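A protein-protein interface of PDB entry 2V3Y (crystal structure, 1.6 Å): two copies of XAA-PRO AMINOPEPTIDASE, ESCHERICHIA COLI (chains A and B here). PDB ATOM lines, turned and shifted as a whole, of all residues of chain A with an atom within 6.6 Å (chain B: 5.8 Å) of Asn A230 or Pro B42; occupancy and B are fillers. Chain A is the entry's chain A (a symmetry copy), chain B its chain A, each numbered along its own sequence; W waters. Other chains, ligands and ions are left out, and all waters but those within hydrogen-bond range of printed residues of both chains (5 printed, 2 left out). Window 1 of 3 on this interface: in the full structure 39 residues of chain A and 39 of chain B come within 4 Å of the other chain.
Among the printed residues, merely in contact across the chains: Asn A230 with Pro B42, Tyr A41 with Tyr B41, Tyr A41 with Arg B44, Arg A35 with Arg B44 and Asn A230 with Tyr B41.
The backbone carbonyl oxygen (O) of Glu B40 sits at hydrogen-bond distance from the side-chain amide nitrogen (ND2) of Asn A230 (3.0 Å). The side-chain hydroxyl (OH) of Tyr A41 lies within hydrogen-bond range of the backbone carbonyl oxygen (O) of Pro B42 (2.7 Å).
Hydrophobic or aromatic side chains of chain B within 4 Å of the printed part of chain A: Tyr B41 and Pro B42. Along chain B the printed residues that touch a printed residue of chain A span positions 40 to 44. Among the printed residues, no Asp or Glu carboxylate lies within 4 Å of a Lys or Arg side-chain nitrogen of the other chain.
Of the printed residues of chain B, Arg A35 touches Arg B44 (3.6 Å). Printed residues of chain A within 4 Å of Glu B40: Asn A230 (3.0 Å). Of the printed residues of chain A, Tyr B41 touches Tyr A41 and Asn A230. Asn A247 touches none of the printed residues of chain B. Tyr A244 touches none of the printed residues of chain B.
Water W1 lies within hydrogen-bond range of OH of Tyr A41 (2.8 Å) and N of Arg B44 (3.1 Å). Water W2 bridges the backbone carbonyl oxygen (O) of Tyr B43 and the guanidinium group (NH2) of Arg A35. Water W4 bridges the backbone NH of Asn A230 (2.9 Å) and the backbone carbonyl oxygen of Glu B40 (3.0 Å). Water W3 lies within hydrogen-bond range of OE2 of Glu A212 and OH of Tyr B226. Water W5 bridges OD1 of Asn A230 (3.1 Å) and O of Glu B40 (3.3 Å).
Tyr A41 touches its own counterpart, Tyr B41.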
ATOM      1  N   ARG A  35      -9.384   4.539  -3.215  1.00  0.00           N
ATOM      2  CA  ARG A  35      -9.331   5.999  -3.240  1.00  0.00           C
ATOM      3  C   ARG A  35     -10.392   6.567  -2.294  1.00  0.00           C
ATOM      4  O   ARG A  35     -10.074   7.374  -1.418  1.00  0.00           O
ATOM      5  CB  ARG A  35      -9.535   6.553  -4.657  1.00  0.00           C
ATOM      6  CG  ARG A  35      -9.477   8.049  -4.722  1.00  0.00           C
ATOM      7  CD  ARG A  35      -9.338   8.591  -6.143  1.00  0.00           C
ATOM      8  NE  ARG A  35      -9.185  10.047  -6.103  1.00  0.00           N
ATOM      9  CZ  ARG A  35     -10.192  10.910  -6.005  1.00  0.00           C
ATOM     10  NH1 ARG A  35     -11.458  10.505  -6.044  1.00  0.00           N
ATOM     11  NH2 ARG A  35      -9.953  12.204  -5.898  1.00  0.00           N
ATOM     12  N   TYR A  41      -7.994   3.675  -6.808  1.00  0.00           N
ATOM     13  CA  TYR A  41      -7.059   4.401  -7.625  1.00  0.00           C
ATOM     14  C   TYR A  41      -6.718   3.527  -8.842  1.00  0.00           C
ATOM     15  O   TYR A  41      -6.827   2.304  -8.766  1.00  0.00           O
ATOM     16  CB  TYR A  41      -5.774   4.642  -6.856  1.00  0.00           C
ATOM     17  CG  TYR A  41      -5.816   5.782  -5.874  1.00  0.00           C
ATOM     18  CD1 TYR A  41      -5.738   7.096  -6.306  1.00  0.00           C
ATOM     19  CD2 TYR A  41      -5.855   5.534  -4.499  1.00  0.00           C
ATOM     20  CE1 TYR A  41      -5.723   8.151  -5.411  1.00  0.00           C
ATOM     21  CE2 TYR A  41      -5.872   6.589  -3.585  1.00  0.00           C
ATOM     22  CZ  TYR A  41      -5.800   7.891  -4.036  1.00  0.00           C
ATOM     23  OH  TYR A  41      -5.806   8.927  -3.126  1.00  0.00           O
ATOM     24  N   GLU A 212      -0.091  21.901 -14.762  1.00  0.00           N
ATOM     25  CA  GLU A 212      -0.264  20.461 -14.504  1.00  0.00           C
ATOM     26  C   GLU A 212      -1.177  19.846 -15.590  1.00  0.00           C
ATOM     27  O   GLU A 212      -0.871  18.807 -16.165  1.00  0.00           O
ATOM     28  CB  GLU A 212      -0.837  20.242 -13.106  1.00  0.00           C
ATOM     29  CG  GLU A 212      -1.313  18.818 -12.847  1.00  0.00           C
ATOM     30  CD  GLU A 212      -1.883  18.661 -11.450  1.00  0.00           C
ATOM     31  OE1 GLU A 212      -1.347  19.307 -10.536  1.00  0.00           O
ATOM     32  OE2 GLU A 212      -2.882  17.922 -11.259  1.00  0.00           O
ATOM     33  N   HIS A 216       0.038  16.854 -18.122  1.00  0.00           N
ATOM     34  CA  HIS A 216      -0.591  15.527 -18.119  1.00  0.00           C
ATOM     35  C   HIS A 216      -1.231  15.171 -19.473  1.00  0.00           C
ATOM     36  O   HIS A 216      -1.213  14.003 -19.889  1.00  0.00           O
ATOM     37  CB  HIS A 216      -1.613  15.471 -17.006  1.00  0.00           C
ATOM     38  CG  HIS A 216      -1.003  15.521 -15.637  1.00  0.00           C
ATOM     39  ND1 HIS A 216      -1.783  15.508 -14.498  1.00  0.00           N
ATOM     40  CD2 HIS A 216       0.283  15.590 -15.221  1.00  0.00           C
ATOM     41  CE1 HIS A 216      -0.989  15.552 -13.436  1.00  0.00           C
ATOM     42  NE2 HIS A 216       0.264  15.591 -13.845  1.00  0.00           N
ATOM     43  N   PRO A 227       1.409  10.171 -14.680  1.00  0.00           N
ATOM     44  CA  PRO A 227       2.720  10.696 -14.228  1.00  0.00           C
ATOM     45  C   PRO A 227       3.447   9.670 -13.355  1.00  0.00           C
ATOM     46  O   PRO A 227       2.804   8.824 -12.732  1.00  0.00           O
ATOM     47  CB  PRO A 227       2.359  11.913 -13.395  1.00  0.00           C
ATOM     48  CG  PRO A 227       0.900  12.174 -13.663  1.00  0.00           C
ATOM     49  CD  PRO A 227       0.275  10.899 -14.062  1.00  0.00           C
ATOM     50  N   SER A 228       4.775   9.751 -13.312  1.00  0.00           N
ATOM     51  CA  SER A 228       5.549   8.867 -12.433  1.00  0.00           C
ATOM     52  C   SER A 228       5.593   9.303 -10.966  1.00  0.00           C
ATOM     53  O   SER A 228       6.021   8.541 -10.084  1.00  0.00           O
ATOM     54  CB  SER A 228       6.996   8.722 -12.979  1.00  0.00           C
ATOM     55  OG  SER A 228       7.575  10.001 -13.138  1.00  0.00           O
ATOM     56  N   TYR A 229       5.080  10.509 -10.694  1.00  0.00           N
ATOM     57  CA  TYR A 229       4.966  11.076  -9.354  1.00  0.00           C
ATOM     58  C   TYR A 229       4.058  12.287  -9.436  1.00  0.00           C
ATOM     59  O   TYR A 229       3.790  12.781 -10.525  1.00  0.00           O
ATOM     60  CB  TYR A 229       6.309  11.461  -8.769  1.00  0.00           C
ATOM     61  CG  TYR A 229       7.073  12.414  -9.629  1.00  0.00           C
ATOM     62  CD1 TYR A 229       7.884  11.935 -10.673  1.00  0.00           C
ATOM     63  CD2 TYR A 229       7.007  13.785  -9.436  1.00  0.00           C
ATOM     64  CE1 TYR A 229       8.576  12.783 -11.509  1.00  0.00           C
ATOM     65  CE2 TYR A 229       7.731  14.668 -10.256  1.00  0.00           C
ATOM     66  CZ  TYR A 229       8.516  14.167 -11.317  1.00  0.00           C
ATOM     67  OH  TYR A 229       9.224  15.007 -12.156  1.00  0.00           O
ATOM     68  N   ASN A 230       3.604  12.769  -8.289  1.00  0.00           N
ATOM     69  CA  ASN A 230       2.688  13.911  -8.273  1.00  0.00           C
ATOM     70  C   ASN A 230       3.398  15.202  -8.716  1.00  0.00           C
ATOM     71  O   ASN A 230       4.363  15.628  -8.122  1.00  0.00           O
ATOM     72  CB  ASN A 230       2.036  14.054  -6.891  1.00  0.00           C
ATOM     73  CG  ASN A 230       1.270  12.782  -6.474  1.00  0.00           C
ATOM     74  OD1 ASN A 230       0.661  12.113  -7.311  1.00  0.00           O
ATOM     75  ND2 ASN A 230       1.252  12.492  -5.188  1.00  0.00           N
ATOM     76  N   THR A 231       2.848  15.796  -9.766  1.00  0.00           N
ATOM     77  CA  THR A 231       3.394  16.992 -10.412  1.00  0.00           C
ATOM     78  C   THR A 231       3.437  18.151  -9.443  1.00  0.00           C
ATOM     79  O   THR A 231       2.434  18.427  -8.754  1.00  0.00           O
ATOM     80  CB  THR A 231       2.493  17.334 -11.626  1.00  0.00           C
ATOM     81  OG1 THR A 231       2.597  16.259 -12.578  1.00  0.00           O
ATOM     82  CG2 THR A 231       2.865  18.659 -12.282  1.00  0.00           C
ATOM     83  N   ILE A 232       4.562  18.865  -9.487  1.00  0.00           N
ATOM     84  CA  ILE A 232       4.861  20.026  -8.648  1.00  0.00           C
ATOM     85  C   ILE A 232       4.865  21.264  -9.551  1.00  0.00           C
ATOM     86  O   ILE A 232       5.632  21.283 -10.519  1.00  0.00           O
ATOM     87  CB  ILE A 232       6.271  19.831  -8.019  1.00  0.00           C
ATOM     88  CG1 ILE A 232       6.228  18.696  -6.981  1.00  0.00           C
ATOM     89  CG2 ILE A 232       6.810  21.124  -7.427  1.00  0.00           C
ATOM     90  CD1 ILE A 232       7.559  17.962  -6.807  1.00  0.00           C
ATOM     91  N   HIS A 243       8.491  19.667  -2.594  1.00  0.00           N
ATOM     92  CA  HIS A 243       7.448  18.783  -3.156  1.00  0.00           C
ATOM     93  C   HIS A 243       6.084  19.453  -3.037  1.00  0.00           C
ATOM     94  O   HIS A 243       5.112  18.839  -2.612  1.00  0.00           O
ATOM     95  CB  HIS A 243       7.453  17.421  -2.453  1.00  0.00           C
ATOM     96  CG  HIS A 243       8.789  16.741  -2.500  1.00  0.00           C
ATOM     97  ND1 HIS A 243       9.741  16.924  -1.519  1.00  0.00           N
ATOM     98  CD2 HIS A 243       9.341  15.903  -3.409  1.00  0.00           C
ATOM     99  CE1 HIS A 243      10.824  16.228  -1.825  1.00  0.00           C
ATOM    100  NE2 HIS A 243      10.608  15.598  -2.962  1.00  0.00           N
ATOM    101  N   TYR A 244       6.025  20.717  -3.433  1.00  0.00           N
ATOM    102  CA  TYR A 244       4.767  21.463  -3.430  1.00  0.00           C
ATOM    103  C   TYR A 244       3.824  20.878  -4.484  1.00  0.00           C
ATOM    104  O   TYR A 244       4.095  20.990  -5.677  1.00  0.00           O
ATOM    105  CB  TYR A 244       5.050  22.936  -3.745  1.00  0.00           C
ATOM    106  CG  TYR A 244       3.794  23.762  -3.915  1.00  0.00           C
ATOM    107  CD1 TYR A 244       3.101  24.261  -2.821  1.00  0.00           C
ATOM    108  CD2 TYR A 244       3.322  24.065  -5.191  1.00  0.00           C
ATOM    109  CE1 TYR A 244       1.956  25.010  -2.983  1.00  0.00           C
ATOM    110  CE2 TYR A 244       2.188  24.829  -5.368  1.00  0.00           C
ATOM    111  CZ  TYR A 244       1.503  25.313  -4.264  1.00  0.00           C
ATOM    112  OH  TYR A 244       0.365  26.077  -4.436  1.00  0.00           O
ATOM    113  N   THR A 245       2.698  20.300  -4.041  1.00  0.00           N
ATOM    114  CA  THR A 245       1.761  19.703  -4.997  1.00  0.00           C
ATOM    115  C   THR A 245       0.342  20.283  -4.890  1.00  0.00           C
ATOM    116  O   THR A 245      -0.541  19.847  -5.638  1.00  0.00           O
ATOM    117  CB  THR A 245       1.705  18.171  -4.834  1.00  0.00           C
ATOM    118  OG1 THR A 245       1.253  17.836  -3.513  1.00  0.00           O
ATOM    119  CG2 THR A 245       3.114  17.545  -5.134  1.00  0.00           C
ATOM    120  N   ASN A 247      -0.611  23.150  -5.893  1.00  0.00           N
ATOM    121  CA  ASN A 247      -0.775  23.714  -7.253  1.00  0.00           C
ATOM    122  C   ASN A 247      -2.055  24.559  -7.356  1.00  0.00           C
ATOM    123  O   ASN A 247      -2.751  24.514  -8.364  1.00  0.00           O
ATOM    124  CB  ASN A 247      -0.750  22.596  -8.301  1.00  0.00           C
ATOM    125  CG  ASN A 247       0.581  21.800  -8.288  1.00  0.00           C
ATOM    126  OD1 ASN A 247       1.537  22.169  -7.581  1.00  0.00           O
ATOM    127  ND2 ASN A 247       0.635  20.699  -9.063  1.00  0.00           N
ATOM    128  N   ASP A 260       8.263  20.505 -11.526  1.00  0.00           N
ATOM    129  CA  ASP A 260       8.936  19.205 -11.405  1.00  0.00           C
ATOM    130  C   ASP A 260       7.866  18.169 -11.773  1.00  0.00           C
ATOM    131  O   ASP A 260       6.872  18.039 -11.071  1.00  0.00           O
ATOM    132  CB  ASP A 260       9.468  19.016  -9.978  1.00  0.00           C
ATOM    133  CG  ASP A 260      10.478  17.868  -9.849  1.00  0.00           C
ATOM    134  OD1 ASP A 260      10.432  16.963 -10.684  1.00  0.00           O
ATOM    135  OD2 ASP A 260      11.259  17.909  -8.884  1.00  0.00           O
ATOM    136  N   ALA A 261       7.998  17.588 -12.961  1.00  0.00           N
ATOM    137  CA  ALA A 261       7.005  16.658 -13.495  1.00  0.00           C
ATOM    138  C   ALA A 261       7.652  15.645 -14.389  1.00  0.00           C
ATOM    139  O   ALA A 261       8.637  15.918 -15.064  1.00  0.00           O
ATOM    140  CB  ALA A 261       5.890  17.406 -14.294  1.00  0.00           C
ATOM    141  N   GLU B  40       3.555   8.387  -3.360  1.00  0.00           N
ATOM    142  CA  GLU B  40       2.176   8.223  -2.933  1.00  0.00           C
ATOM    143  C   GLU B  40       1.221   8.709  -4.018  1.00  0.00           C
ATOM    144  O   GLU B  40       1.588   9.548  -4.861  1.00  0.00           O
ATOM    145  CB  GLU B  40       1.937   8.992  -1.629  1.00  0.00           C
ATOM    146  CG  GLU B  40       2.774   8.478  -0.448  1.00  0.00           C
ATOM    147  CD  GLU B  40       2.807   9.453   0.717  1.00  0.00           C
ATOM    148  OE1 GLU B  40       1.908  10.310   0.783  1.00  0.00           O
ATOM    149  OE2 GLU B  40       3.737   9.374   1.547  1.00  0.00           O
ATOM    150  N   TYR B  41      -0.001   8.176  -3.997  1.00  0.00           N
ATOM    151  CA  TYR B  41      -1.048   8.686  -4.841  1.00  0.00           C
ATOM    152  C   TYR B  41      -1.436  10.079  -4.321  1.00  0.00           C
ATOM    153  O   TYR B  41      -1.242  10.367  -3.141  1.00  0.00           O
ATOM    154  CB  TYR B  41      -2.275   7.800  -4.742  1.00  0.00           C
ATOM    155  CG  TYR B  41      -2.221   6.535  -5.556  1.00  0.00           C
ATOM    156  CD1 TYR B  41      -2.422   6.562  -6.926  1.00  0.00           C
ATOM    157  CD2 TYR B  41      -2.048   5.295  -4.934  1.00  0.00           C
ATOM    158  CE1 TYR B  41      -2.426   5.401  -7.679  1.00  0.00           C
ATOM    159  CE2 TYR B  41      -2.019   4.119  -5.684  1.00  0.00           C
ATOM    160  CZ  TYR B  41      -2.214   4.169  -7.049  1.00  0.00           C
ATOM    161  OH  TYR B  41      -2.196   3.000  -7.781  1.00  0.00           O
ATOM    162  N   PRO B  42      -1.982  10.918  -5.206  1.00  0.00           N
ATOM    163  CA  PRO B  42      -2.516  12.210  -4.746  1.00  0.00           C
ATOM    164  C   PRO B  42      -3.521  11.971  -3.633  1.00  0.00           C
ATOM    165  O   PRO B  42      -4.386  11.091  -3.742  1.00  0.00           O
ATOM    166  CB  PRO B  42      -3.232  12.768  -5.971  1.00  0.00           C
ATOM    167  CG  PRO B  42      -2.599  12.098  -7.145  1.00  0.00           C
ATOM    168  CD  PRO B  42      -2.223  10.703  -6.637  1.00  0.00           C
ATOM    169  N   TYR B  43      -3.435  12.769  -2.585  1.00  0.00           N
ATOM    170  CA  TYR B  43      -4.228  12.524  -1.382  1.00  0.00           C
ATOM    171  C   TYR B  43      -5.706  12.743  -1.664  1.00  0.00           C
ATOM    172  O   TYR B  43      -6.098  13.722  -2.338  1.00  0.00           O
ATOM    173  CB  TYR B  43      -3.790  13.453  -0.257  1.00  0.00           C
ATOM    174  CG  TYR B  43      -4.479  13.186   1.046  1.00  0.00           C
ATOM    175  CD1 TYR B  43      -4.275  11.981   1.714  1.00  0.00           C
ATOM    176  CD2 TYR B  43      -5.361  14.113   1.615  1.00  0.00           C
ATOM    177  CE1 TYR B  43      -4.911  11.686   2.912  1.00  0.00           C
ATOM    178  CE2 TYR B  43      -5.994  13.841   2.798  1.00  0.00           C
ATOM    179  CZ  TYR B  43      -5.779  12.628   3.473  1.00  0.00           C
ATOM    180  OH  TYR B  43      -6.414  12.354   4.682  1.00  0.00           O
ATOM    181  N   ARG B  44      -6.520  11.817  -1.167  1.00  0.00           N
ATOM    182  CA  ARG B  44      -7.989  11.974  -1.208  1.00  0.00           C
ATOM    183  C   ARG B  44      -8.509  11.845   0.215  1.00  0.00           C
ATOM    184  O   ARG B  44      -8.414  10.765   0.832  1.00  0.00           O
ATOM    185  CB  ARG B  44      -8.635  10.919  -2.133  1.00  0.00           C
ATOM    186  CG  ARG B  44     -10.172  10.901  -2.098  1.00  0.00           C
ATOM    187  CD  ARG B  44     -10.853  12.279  -2.231  1.00  0.00           C
ATOM    188  NE  ARG B  44     -12.139  12.064  -2.898  1.00  0.00           N
ATOM    189  CZ  ARG B  44     -13.202  11.490  -2.334  1.00  0.00           C
ATOM    190  NH1 ARG B  44     -13.192  11.181  -1.040  1.00  0.00           N
ATOM    191  NH2 ARG B  44     -14.310  11.251  -3.048  1.00  0.00           N
ATOM    192  N   TYR B 226      -9.008  16.330 -10.453  1.00  0.00           N
ATOM    193  CA  TYR B 226      -9.048  14.861 -10.501  1.00  0.00           C
ATOM    194  C   TYR B 226     -10.423  14.354 -10.924  1.00  0.00           C
ATOM    195  O   TYR B 226     -11.458  14.963 -10.576  1.00  0.00           O
ATOM    196  CB  TYR B 226      -8.724  14.262  -9.133  1.00  0.00           C
ATOM    197  CG  TYR B 226      -7.396  14.729  -8.566  1.00  0.00           C
ATOM    198  CD1 TYR B 226      -6.222  14.439  -9.213  1.00  0.00           C
ATOM    199  CD2 TYR B 226      -7.348  15.480  -7.401  1.00  0.00           C
ATOM    200  CE1 TYR B 226      -4.999  14.902  -8.702  1.00  0.00           C
ATOM    201  CE2 TYR B 226      -6.150  15.936  -6.899  1.00  0.00           C
ATOM    202  CZ  TYR B 226      -4.986  15.624  -7.551  1.00  0.00           C
ATOM    203  OH  TYR B 226      -3.786  16.100  -7.047  1.00  0.00           O
HETATM  204  O   HOH W   1      -5.030   9.222  -0.484  1.00  0.00           O
HETATM  205  O   HOH W   2      -7.325  13.362  -4.847  1.00  0.00           O
HETATM  206  O   HOH W   3      -1.739  16.083  -9.255  1.00  0.00           O
HETATM  207  O   HOH W   4       3.930  10.882  -6.073  1.00  0.00           O
HETATM  208  O   HOH W   5       1.830   9.355  -8.154  1.00  0.00           O
